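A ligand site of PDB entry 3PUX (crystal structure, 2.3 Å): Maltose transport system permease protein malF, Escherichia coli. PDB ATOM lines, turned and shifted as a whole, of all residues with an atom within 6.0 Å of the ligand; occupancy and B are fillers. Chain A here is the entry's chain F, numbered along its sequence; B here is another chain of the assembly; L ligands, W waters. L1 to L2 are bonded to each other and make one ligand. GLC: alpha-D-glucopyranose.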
ATOM      1  N   THR A 291      12.993  -4.544 -24.860  1.00  0.00           N
ATOM      2  CA  THR A 291      11.827  -5.288 -24.410  1.00  0.00           C
ATOM      3  C   THR A 291      10.562  -4.483 -24.687  1.00  0.00           C
ATOM      4  O   THR A 291       9.659  -4.946 -25.358  1.00  0.00           O
ATOM      5  CB  THR A 291      11.908  -5.616 -22.888  1.00  0.00           C
ATOM      6  OG1 THR A 291      13.079  -6.405 -22.616  1.00  0.00           O
ATOM      7  CG2 THR A 291      10.645  -6.361 -22.385  1.00  0.00           C
ATOM      8  N   VAL A 292      10.518  -3.263 -24.159  1.00  0.00           N
ATOM      9  CA  VAL A 292       9.375  -2.383 -24.381  1.00  0.00           C
ATOM     10  C   VAL A 292       9.065  -2.234 -25.868  1.00  0.00           C
ATOM     11  O   VAL A 292       7.945  -2.460 -26.301  1.00  0.00           O
ATOM     12  CB  VAL A 292       9.572  -1.022 -23.669  1.00  0.00           C
ATOM     13  CG1 VAL A 292       8.534  -0.018 -24.116  1.00  0.00           C
ATOM     14  CG2 VAL A 292       9.458  -1.198 -22.161  1.00  0.00           C
ATOM     15  N   THR A 295       7.852  -5.651 -27.415  1.00  0.00           N
ATOM     16  CA  THR A 295       6.541  -6.024 -26.869  1.00  0.00           C
ATOM     17  C   THR A 295       5.426  -5.117 -27.379  1.00  0.00           C
ATOM     18  O   THR A 295       4.374  -5.601 -27.778  1.00  0.00           O
ATOM     19  CB  THR A 295       6.532  -6.150 -25.329  1.00  0.00           C
ATOM     20  OG1 THR A 295       7.010  -4.927 -24.730  1.00  0.00           O
ATOM     21  CG2 THR A 295       7.418  -7.308 -24.897  1.00  0.00           C
ATOM     22  N   TYR A 325       0.507 -15.551 -21.120  1.00  0.00           N
ATOM     23  CA  TYR A 325       0.294 -14.670 -19.980  1.00  0.00           C
ATOM     24  C   TYR A 325      -0.715 -15.281 -19.012  1.00  0.00           C
ATOM     25  O   TYR A 325      -0.832 -14.829 -17.869  1.00  0.00           O
ATOM     26  CB  TYR A 325      -0.199 -13.324 -20.503  1.00  0.00           C
ATOM     27  CG  TYR A 325      -0.157 -12.146 -19.556  1.00  0.00           C
ATOM     28  CD1 TYR A 325       0.777 -12.070 -18.493  1.00  0.00           C
ATOM     29  CD2 TYR A 325      -1.014 -11.055 -19.755  1.00  0.00           C
ATOM     30  CE1 TYR A 325       0.812 -10.926 -17.646  1.00  0.00           C
ATOM     31  CE2 TYR A 325      -0.982  -9.941 -18.931  1.00  0.00           C
ATOM     32  CZ  TYR A 325      -0.082  -9.874 -17.889  1.00  0.00           C
ATOM     33  OH  TYR A 325      -0.103  -8.749 -17.117  1.00  0.00           O
ATOM     34  N   SER A 329       4.389 -17.264 -15.012  1.00  0.00           N
ATOM     35  CA  SER A 329       5.649 -17.106 -15.733  1.00  0.00           C
ATOM     36  C   SER A 329       6.770 -17.995 -15.194  1.00  0.00           C
ATOM     37  O   SER A 329       7.622 -18.451 -15.945  1.00  0.00           O
ATOM     38  CB  SER A 329       6.062 -15.642 -15.684  1.00  0.00           C
ATOM     39  OG  SER A 329       6.272 -15.288 -14.325  1.00  0.00           O
ATOM     40  N   ILE A 333       9.572 -19.762 -17.520  1.00  0.00           N
ATOM     41  CA  ILE A 333      10.959 -19.315 -17.545  1.00  0.00           C
ATOM     42  C   ILE A 333      11.905 -20.512 -17.395  1.00  0.00           C
ATOM     43  O   ILE A 333      12.884 -20.663 -18.150  1.00  0.00           O
ATOM     44  CB  ILE A 333      11.202 -18.268 -16.433  1.00  0.00           C
ATOM     45  CG1 ILE A 333      10.471 -16.971 -16.779  1.00  0.00           C
ATOM     46  CG2 ILE A 333      12.683 -17.979 -16.284  1.00  0.00           C
ATOM     47  CD1 ILE A 333      10.354 -15.989 -15.602  1.00  0.00           C
ATOM     48  N   ASN A 376      11.795 -12.628 -22.659  1.00  0.00           N
ATOM     49  CA  ASN A 376      11.060 -11.470 -22.176  1.00  0.00           C
ATOM     50  C   ASN A 376       9.930 -11.006 -23.106  1.00  0.00           C
ATOM     51  O   ASN A 376       8.822 -10.726 -22.651  1.00  0.00           O
ATOM     52  CB  ASN A 376      12.000 -10.319 -21.818  1.00  0.00           C
ATOM     53  CG  ASN A 376      11.541  -9.557 -20.594  1.00  0.00           C
ATOM     54  OD1 ASN A 376      10.695 -10.051 -19.850  1.00  0.00           O
ATOM     55  ND2 ASN A 376      12.088  -8.388 -20.378  1.00  0.00           N
ATOM     56  N   THR A 377      10.214 -10.932 -24.393  1.00  0.00           N
ATOM     57  CA  THR A 377       9.210 -10.601 -25.416  1.00  0.00           C
ATOM     58  C   THR A 377       8.011 -11.573 -25.424  1.00  0.00           C
ATOM     59  O   THR A 377       6.862 -11.164 -25.661  1.00  0.00           O
ATOM     60  CB  THR A 377       9.841 -10.588 -26.826  1.00  0.00           C
ATOM     61  OG1 THR A 377      10.937  -9.648 -26.876  1.00  0.00           O
ATOM     62  CG2 THR A 377       8.810 -10.224 -27.899  1.00  0.00           C
ATOM     63  N   LEU A 379       7.063 -13.387 -22.789  1.00  0.00           N
ATOM     64  CA  LEU A 379       6.320 -13.055 -21.566  1.00  0.00           C
ATOM     65  C   LEU A 379       5.510 -11.758 -21.693  1.00  0.00           C
ATOM     66  O   LEU A 379       4.412 -11.652 -21.155  1.00  0.00           O
ATOM     67  CB  LEU A 379       7.290 -12.926 -20.378  1.00  0.00           C
ATOM     68  CG  LEU A 379       8.139 -14.104 -19.886  1.00  0.00           C
ATOM     69  CD1 LEU A 379       9.157 -13.600 -18.858  1.00  0.00           C
ATOM     70  CD2 LEU A 379       7.260 -15.173 -19.287  1.00  0.00           C
ATOM     71  N   GLY A 380       6.033 -10.763 -22.413  1.00  0.00           N
ATOM     72  CA  GLY A 380       5.479  -9.391 -22.332  1.00  0.00           C
ATOM     73  C   GLY A 380       4.545  -8.918 -23.441  1.00  0.00           C
ATOM     74  O   GLY A 380       3.838  -7.929 -23.271  1.00  0.00           O
ATOM     75  N   TYR A 381       4.543  -9.618 -24.568  1.00  0.00           N
ATOM     76  CA  TYR A 381       3.723  -9.189 -25.698  1.00  0.00           C
ATOM     77  C   TYR A 381       2.193  -9.252 -25.442  1.00  0.00           C
ATOM     78  O   TYR A 381       1.476  -8.386 -25.927  1.00  0.00           O
ATOM     79  CB  TYR A 381       4.125  -9.872 -27.028  1.00  0.00           C
ATOM     80  CG  TYR A 381       3.482 -11.229 -27.290  1.00  0.00           C
ATOM     81  CD1 TYR A 381       2.157 -11.322 -27.724  1.00  0.00           C
ATOM     82  CD2 TYR A 381       4.209 -12.393 -27.126  1.00  0.00           C
ATOM     83  CE1 TYR A 381       1.554 -12.551 -27.974  1.00  0.00           C
ATOM     84  CE2 TYR A 381       3.633 -13.646 -27.367  1.00  0.00           C
ATOM     85  CZ  TYR A 381       2.310 -13.718 -27.793  1.00  0.00           C
ATOM     86  OH  TYR A 381       1.734 -14.948 -27.994  1.00  0.00           O
ATOM     87  N   TYR A 383       0.466  -8.583 -22.770  1.00  0.00           N
ATOM     88  CA  TYR A 383       0.127  -7.393 -22.018  1.00  0.00           C
ATOM     89  C   TYR A 383      -0.049  -6.216 -22.970  1.00  0.00           C
ATOM     90  O   TYR A 383      -1.071  -5.519 -22.912  1.00  0.00           O
ATOM     91  CB  TYR A 383       1.253  -7.102 -21.018  1.00  0.00           C
ATOM     92  CG  TYR A 383       1.097  -5.811 -20.252  1.00  0.00           C
ATOM     93  CD1 TYR A 383       0.092  -5.665 -19.298  1.00  0.00           C
ATOM     94  CD2 TYR A 383       1.962  -4.741 -20.473  1.00  0.00           C
ATOM     95  CE1 TYR A 383      -0.055  -4.470 -18.585  1.00  0.00           C
ATOM     96  CE2 TYR A 383       1.829  -3.530 -19.752  1.00  0.00           C
ATOM     97  CZ  TYR A 383       0.835  -3.411 -18.805  1.00  0.00           C
ATOM     98  OH  TYR A 383       0.683  -2.227 -18.098  1.00  0.00           O
ATOM     99  N   MET A 384       0.921  -5.990 -23.855  1.00  0.00           N
ATOM    100  CA  MET A 384       0.831  -4.898 -24.806  1.00  0.00           C
ATOM    101  C   MET A 384      -0.241  -5.139 -25.819  1.00  0.00           C
ATOM    102  O   MET A 384      -0.929  -4.193 -26.214  1.00  0.00           O
ATOM    103  CB  MET A 384       2.155  -4.663 -25.496  1.00  0.00           C
ATOM    104  CG  MET A 384       3.177  -4.032 -24.607  1.00  0.00           C
ATOM    105  SD  MET A 384       2.621  -2.442 -23.961  1.00  0.00           S
ATOM    106  CE  MET A 384       3.978  -2.114 -22.828  1.00  0.00           C
ATOM    107  N   LEU A 429       1.936   3.923 -20.369  1.00  0.00           N
ATOM    108  CA  LEU A 429       2.150   2.472 -20.243  1.00  0.00           C
ATOM    109  C   LEU A 429       3.539   2.009 -20.675  1.00  0.00           C
ATOM    110  O   LEU A 429       4.096   1.080 -20.088  1.00  0.00           O
ATOM    111  CB  LEU A 429       1.080   1.677 -20.962  1.00  0.00           C
ATOM    112  CG  LEU A 429      -0.299   2.026 -20.416  1.00  0.00           C
ATOM    113  CD1 LEU A 429      -1.411   1.696 -21.416  1.00  0.00           C
ATOM    114  CD2 LEU A 429      -0.543   1.376 -19.041  1.00  0.00           C
ATOM    115  N   ALA A 432       6.146   3.150 -18.067  1.00  0.00           N
ATOM    116  CA  ALA A 432       6.013   2.295 -16.890  1.00  0.00           C
ATOM    117  C   ALA A 432       6.616   0.918 -17.134  1.00  0.00           C
ATOM    118  O   ALA A 432       7.220   0.308 -16.250  1.00  0.00           O
ATOM    119  CB  ALA A 432       4.583   2.182 -16.520  1.00  0.00           C
ATOM    120  N   SER A 433       6.451   0.427 -18.357  1.00  0.00           N
ATOM    121  CA  SER A 433       6.988  -0.874 -18.710  1.00  0.00           C
ATOM    122  C   SER A 433       8.510  -0.835 -18.705  1.00  0.00           C
ATOM    123  O   SER A 433       9.147  -1.831 -18.427  1.00  0.00           O
ATOM    124  CB  SER A 433       6.457  -1.323 -20.081  1.00  0.00           C
ATOM    125  OG  SER A 433       6.972  -2.589 -20.438  1.00  0.00           O
ATOM    126  N   PHE A 434       9.073   0.326 -19.020  1.00  0.00           N
ATOM    127  CA  PHE A 434      10.512   0.542 -18.929  1.00  0.00           C
ATOM    128  C   PHE A 434      11.006   0.432 -17.492  1.00  0.00           C
ATOM    129  O   PHE A 434      12.024  -0.204 -17.258  1.00  0.00           O
ATOM    130  CB  PHE A 434      10.903   1.894 -19.511  1.00  0.00           C
ATOM    131  CG  PHE A 434      12.327   2.267 -19.259  1.00  0.00           C
ATOM    132  CD1 PHE A 434      12.674   2.978 -18.100  1.00  0.00           C
ATOM    133  CD2 PHE A 434      13.329   1.899 -20.140  1.00  0.00           C
ATOM    134  CE1 PHE A 434      13.997   3.315 -17.841  1.00  0.00           C
ATOM    135  CE2 PHE A 434      14.658   2.230 -19.892  1.00  0.00           C
ATOM    136  CZ  PHE A 434      14.992   2.947 -18.735  1.00  0.00           C
ATOM    137  N   PHE A 436       9.482  -1.124 -14.947  1.00  0.00           N
ATOM    138  CA  PHE A 436       9.253  -2.478 -14.469  1.00  0.00           C
ATOM    139  C   PHE A 436      10.349  -3.409 -14.993  1.00  0.00           C
ATOM    140  O   PHE A 436      10.859  -4.239 -14.252  1.00  0.00           O
ATOM    141  CB  PHE A 436       7.867  -2.971 -14.895  1.00  0.00           C
ATOM    142  CG  PHE A 436       7.638  -4.456 -14.658  1.00  0.00           C
ATOM    143  CD1 PHE A 436       8.002  -5.403 -15.623  1.00  0.00           C
ATOM    144  CD2 PHE A 436       7.020  -4.886 -13.490  1.00  0.00           C
ATOM    145  CE1 PHE A 436       7.794  -6.761 -15.412  1.00  0.00           C
ATOM    146  CE2 PHE A 436       6.805  -6.254 -13.251  1.00  0.00           C
ATOM    147  CZ  PHE A 436       7.175  -7.185 -14.220  1.00  0.00           C
ATOM    148  N   ASN A 437      10.705  -3.273 -16.262  1.00  0.00           N
ATOM    149  CA  ASN A 437      11.704  -4.154 -16.846  1.00  0.00           C
ATOM    150  C   ASN A 437      13.117  -3.809 -16.411  1.00  0.00           C
ATOM    151  O   ASN A 437      13.976  -4.690 -16.333  1.00  0.00           O
ATOM    152  CB  ASN A 437      11.597  -4.164 -18.364  1.00  0.00           C
ATOM    153  CG  ASN A 437      10.522  -5.100 -18.840  1.00  0.00           C
ATOM    154  OD1 ASN A 437       9.575  -4.683 -19.516  1.00  0.00           O
ATOM    155  ND2 ASN A 437      10.645  -6.367 -18.487  1.00  0.00           N
ATOM    156  N   ASN A 440      13.571  -5.973 -13.459  1.00  0.00           N
ATOM    157  CA  ASN A 440      13.094  -7.342 -13.642  1.00  0.00           C
ATOM    158  C   ASN A 440      14.065  -8.387 -13.063  1.00  0.00           C
ATOM    159  O   ASN A 440      14.602  -9.249 -13.783  1.00  0.00           O
ATOM    160  CB  ASN A 440      12.810  -7.587 -15.122  1.00  0.00           C
ATOM    161  CG  ASN A 440      11.666  -8.581 -15.352  1.00  0.00           C
ATOM    162  OD1 ASN A 440      10.981  -8.531 -16.388  1.00  0.00           O
ATOM    163  ND2 ASN A 440      11.465  -9.491 -14.395  1.00  0.00           N
ATOM    164  N   LEU A 443      13.398 -12.564 -13.727  1.00  0.00           N
ATOM    165  CA  LEU A 443      13.729 -13.189 -15.010  1.00  0.00           C
ATOM    166  C   LEU A 443      15.204 -13.571 -15.110  1.00  0.00           C
ATOM    167  O   LEU A 443      15.509 -14.725 -15.433  1.00  0.00           O
ATOM    168  CB  LEU A 443      13.341 -12.299 -16.179  1.00  0.00           C
ATOM    169  CG  LEU A 443      13.746 -12.727 -17.581  1.00  0.00           C
ATOM    170  CD1 LEU A 443      13.143 -14.059 -18.009  1.00  0.00           C
ATOM    171  CD2 LEU A 443      13.316 -11.649 -18.542  1.00  0.00           C
ATOM    172  N   LEU B 172      -1.893   2.745 -12.968  1.00  0.00           N
ATOM    173  CA  LEU B 172      -1.686   2.568 -14.383  1.00  0.00           C
ATOM    174  C   LEU B 172      -3.018   2.442 -15.102  1.00  0.00           C
ATOM    175  O   LEU B 172      -3.192   2.965 -16.219  1.00  0.00           O
ATOM    176  CB  LEU B 172      -0.777   1.354 -14.639  1.00  0.00           C
ATOM    177  CG  LEU B 172       0.724   1.672 -14.573  1.00  0.00           C
ATOM    178  CD1 LEU B 172       1.587   0.437 -14.651  1.00  0.00           C
ATOM    179  CD2 LEU B 172       1.081   2.643 -15.677  1.00  0.00           C
ATOM    180  N   LEU B 221      -6.670  -7.316 -17.442  1.00  0.00           N
ATOM    181  CA  LEU B 221      -5.321  -7.134 -16.917  1.00  0.00           C
ATOM    182  C   LEU B 221      -5.263  -7.303 -15.398  1.00  0.00           C
ATOM    183  O   LEU B 221      -4.243  -7.721 -14.858  1.00  0.00           O
ATOM    184  CB  LEU B 221      -4.771  -5.791 -17.313  1.00  0.00           C
ATOM    185  CG  LEU B 221      -4.329  -5.692 -18.781  1.00  0.00           C
ATOM    186  CD1 LEU B 221      -3.734  -4.324 -19.016  1.00  0.00           C
ATOM    187  CD2 LEU B 221      -3.311  -6.801 -19.224  1.00  0.00           C
ATOM    188  N   ALA B 225      -3.378 -10.490 -13.217  1.00  0.00           N
ATOM    189  CA  ALA B 225      -2.486 -10.086 -12.145  1.00  0.00           C
ATOM    190  C   ALA B 225      -2.832 -10.840 -10.853  1.00  0.00           C
ATOM    191  O   ALA B 225      -1.937 -11.396 -10.206  1.00  0.00           O
ATOM    192  CB  ALA B 225      -2.575  -8.605 -11.938  1.00  0.00           C
HETATM  193  C1  GLC L   1       2.528  -4.610 -15.425  1.00  0.00           C
HETATM  194  C2  GLC L   1       1.872  -5.996 -15.591  1.00  0.00           C
HETATM  195  C3  GLC L   1       2.897  -7.090 -15.853  1.00  0.00           C
HETATM  196  C4  GLC L   1       3.843  -6.742 -17.006  1.00  0.00           C
HETATM  197  C5  GLC L   1       4.474  -5.372 -16.818  1.00  0.00           C
HETATM  198  C6  GLC L   1       5.007  -5.004 -18.214  1.00  0.00           C
HETATM  199  O1  GLC L   1       3.037  -4.428 -14.099  1.00  0.00           O
HETATM  200  O2  GLC L   1       1.125  -6.402 -14.434  1.00  0.00           O
HETATM  201  O3  GLC L   1       2.176  -8.285 -16.185  1.00  0.00           O
HETATM  202  O4  GLC L   1       4.904  -7.700 -17.070  1.00  0.00           O
HETATM  203  O5  GLC L   1       3.569  -4.345 -16.388  1.00  0.00           O
HETATM  204  O6  GLC L   1       5.490  -3.657 -18.244  1.00  0.00           O
HETATM  205  C1  GLC L   2       4.762  -8.665 -18.107  1.00  0.00           C
HETATM  206  C2  GLC L   2       5.051 -10.053 -17.506  1.00  0.00           C
HETATM  207  C3  GLC L   2       6.510 -10.153 -17.097  1.00  0.00           C
HETATM  208  C4  GLC L   2       7.440  -9.755 -18.257  1.00  0.00           C
HETATM  209  C5  GLC L   2       7.016  -8.400 -18.826  1.00  0.00           C
HETATM  210  C6  GLC L   2       7.848  -7.929 -20.005  1.00  0.00           C
HETATM  211  O2  GLC L   2       4.239 -10.241 -16.352  1.00  0.00           O
HETATM  212  O3  GLC L   2       6.800 -11.481 -16.650  1.00  0.00           O
HETATM  213  O4  GLC L   2       8.789  -9.720 -17.773  1.00  0.00           O
HETATM  214  O5  GLC L   2       5.638  -8.413 -19.222  1.00  0.00           O
HETATM  215  O6  GLC L   2       7.712  -6.501 -20.077  1.00  0.00           O
HETATM  216  O   HOH W   1       9.406 -11.139 -15.726  1.00  0.00           O
HETATM  217  O   HOH W   2       3.753  -1.086 -18.249  1.00  0.00           O
HETATM  218  O   HOH W   3      -1.491  -7.595 -15.388  1.00  0.00           O
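The side-chain amide oxygen (OD1) of Asn 376 sits at hydrogen-bond distance from an oxygen (O4) of GLC L2, at 2.8 Å.
OD1 of Asn 440 is in hydrogen-bond range of O4 of GLC L2 (2.9 Å).
The side-chain hydroxyl (OG) of Ser 433 is in hydrogen-bond range of an oxygen (O6) of GLC L1 (2.9 Å).
OD1 of Asn 437 lies within hydrogen-bond range of O6 of GLC L2 (2.7 Å).
An oxygen (O3) of GLC L1 is in hydrogen-bond range of the side-chain hydroxyl (OH) of Tyr 325, at 2.5 Å.
The side-chain amide oxygen (OD1) of Asn 440 sits at hydrogen-bond distance from the side-chain amide nitrogen (ND2) of Asn 437, at 3.0 Å.
ND2 of Asn 437 sits close to ND2 of Asn 376 (3.1 Å).
The backbone carbonyl oxygen (O) of Ser 433 sits close to the side-chain amide oxygen (OD1) of Asn 437, 3.1 Å away.
The backbone carbonyl oxygen of Thr 291 is in hydrogen-bond range of the side-chain hydroxyl of Thr 295, 2.7 Å away.
ND2 of Asn 376 sits at hydrogen-bond distance from OG1 of Thr 291 (3.2 Å).
Merely in contact with the ligand: Thr 291 (3.7 Å), Leu 379 (3.8 Å), Gly 380 (3.3 Å), Tyr 383 (3.8 Å) and Phe 436 (3.5 Å).
Of the 24 residues printed, 10 come within 4 Å of the ligand.
Water W1 bridges an oxygen (O4) of GLC L2 and the side-chain amide nitrogen of Asn 440.
Water W3 lies within hydrogen-bond range of the side-chain hydroxyl of Tyr 325 (2.5 Å), the backbone carbonyl oxygen of Leu 221 of chain B (2.8 Å) and an oxygen (O2) of GLC L1 (3.0 Å).
Water W2 lies within hydrogen-bond range of O of Leu 429 (2.9 Å), N of Ser 433 (3.1 Å), O6 of GLC L1 (3.1 Å) and OH of Tyr 383 (3.3 Å).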
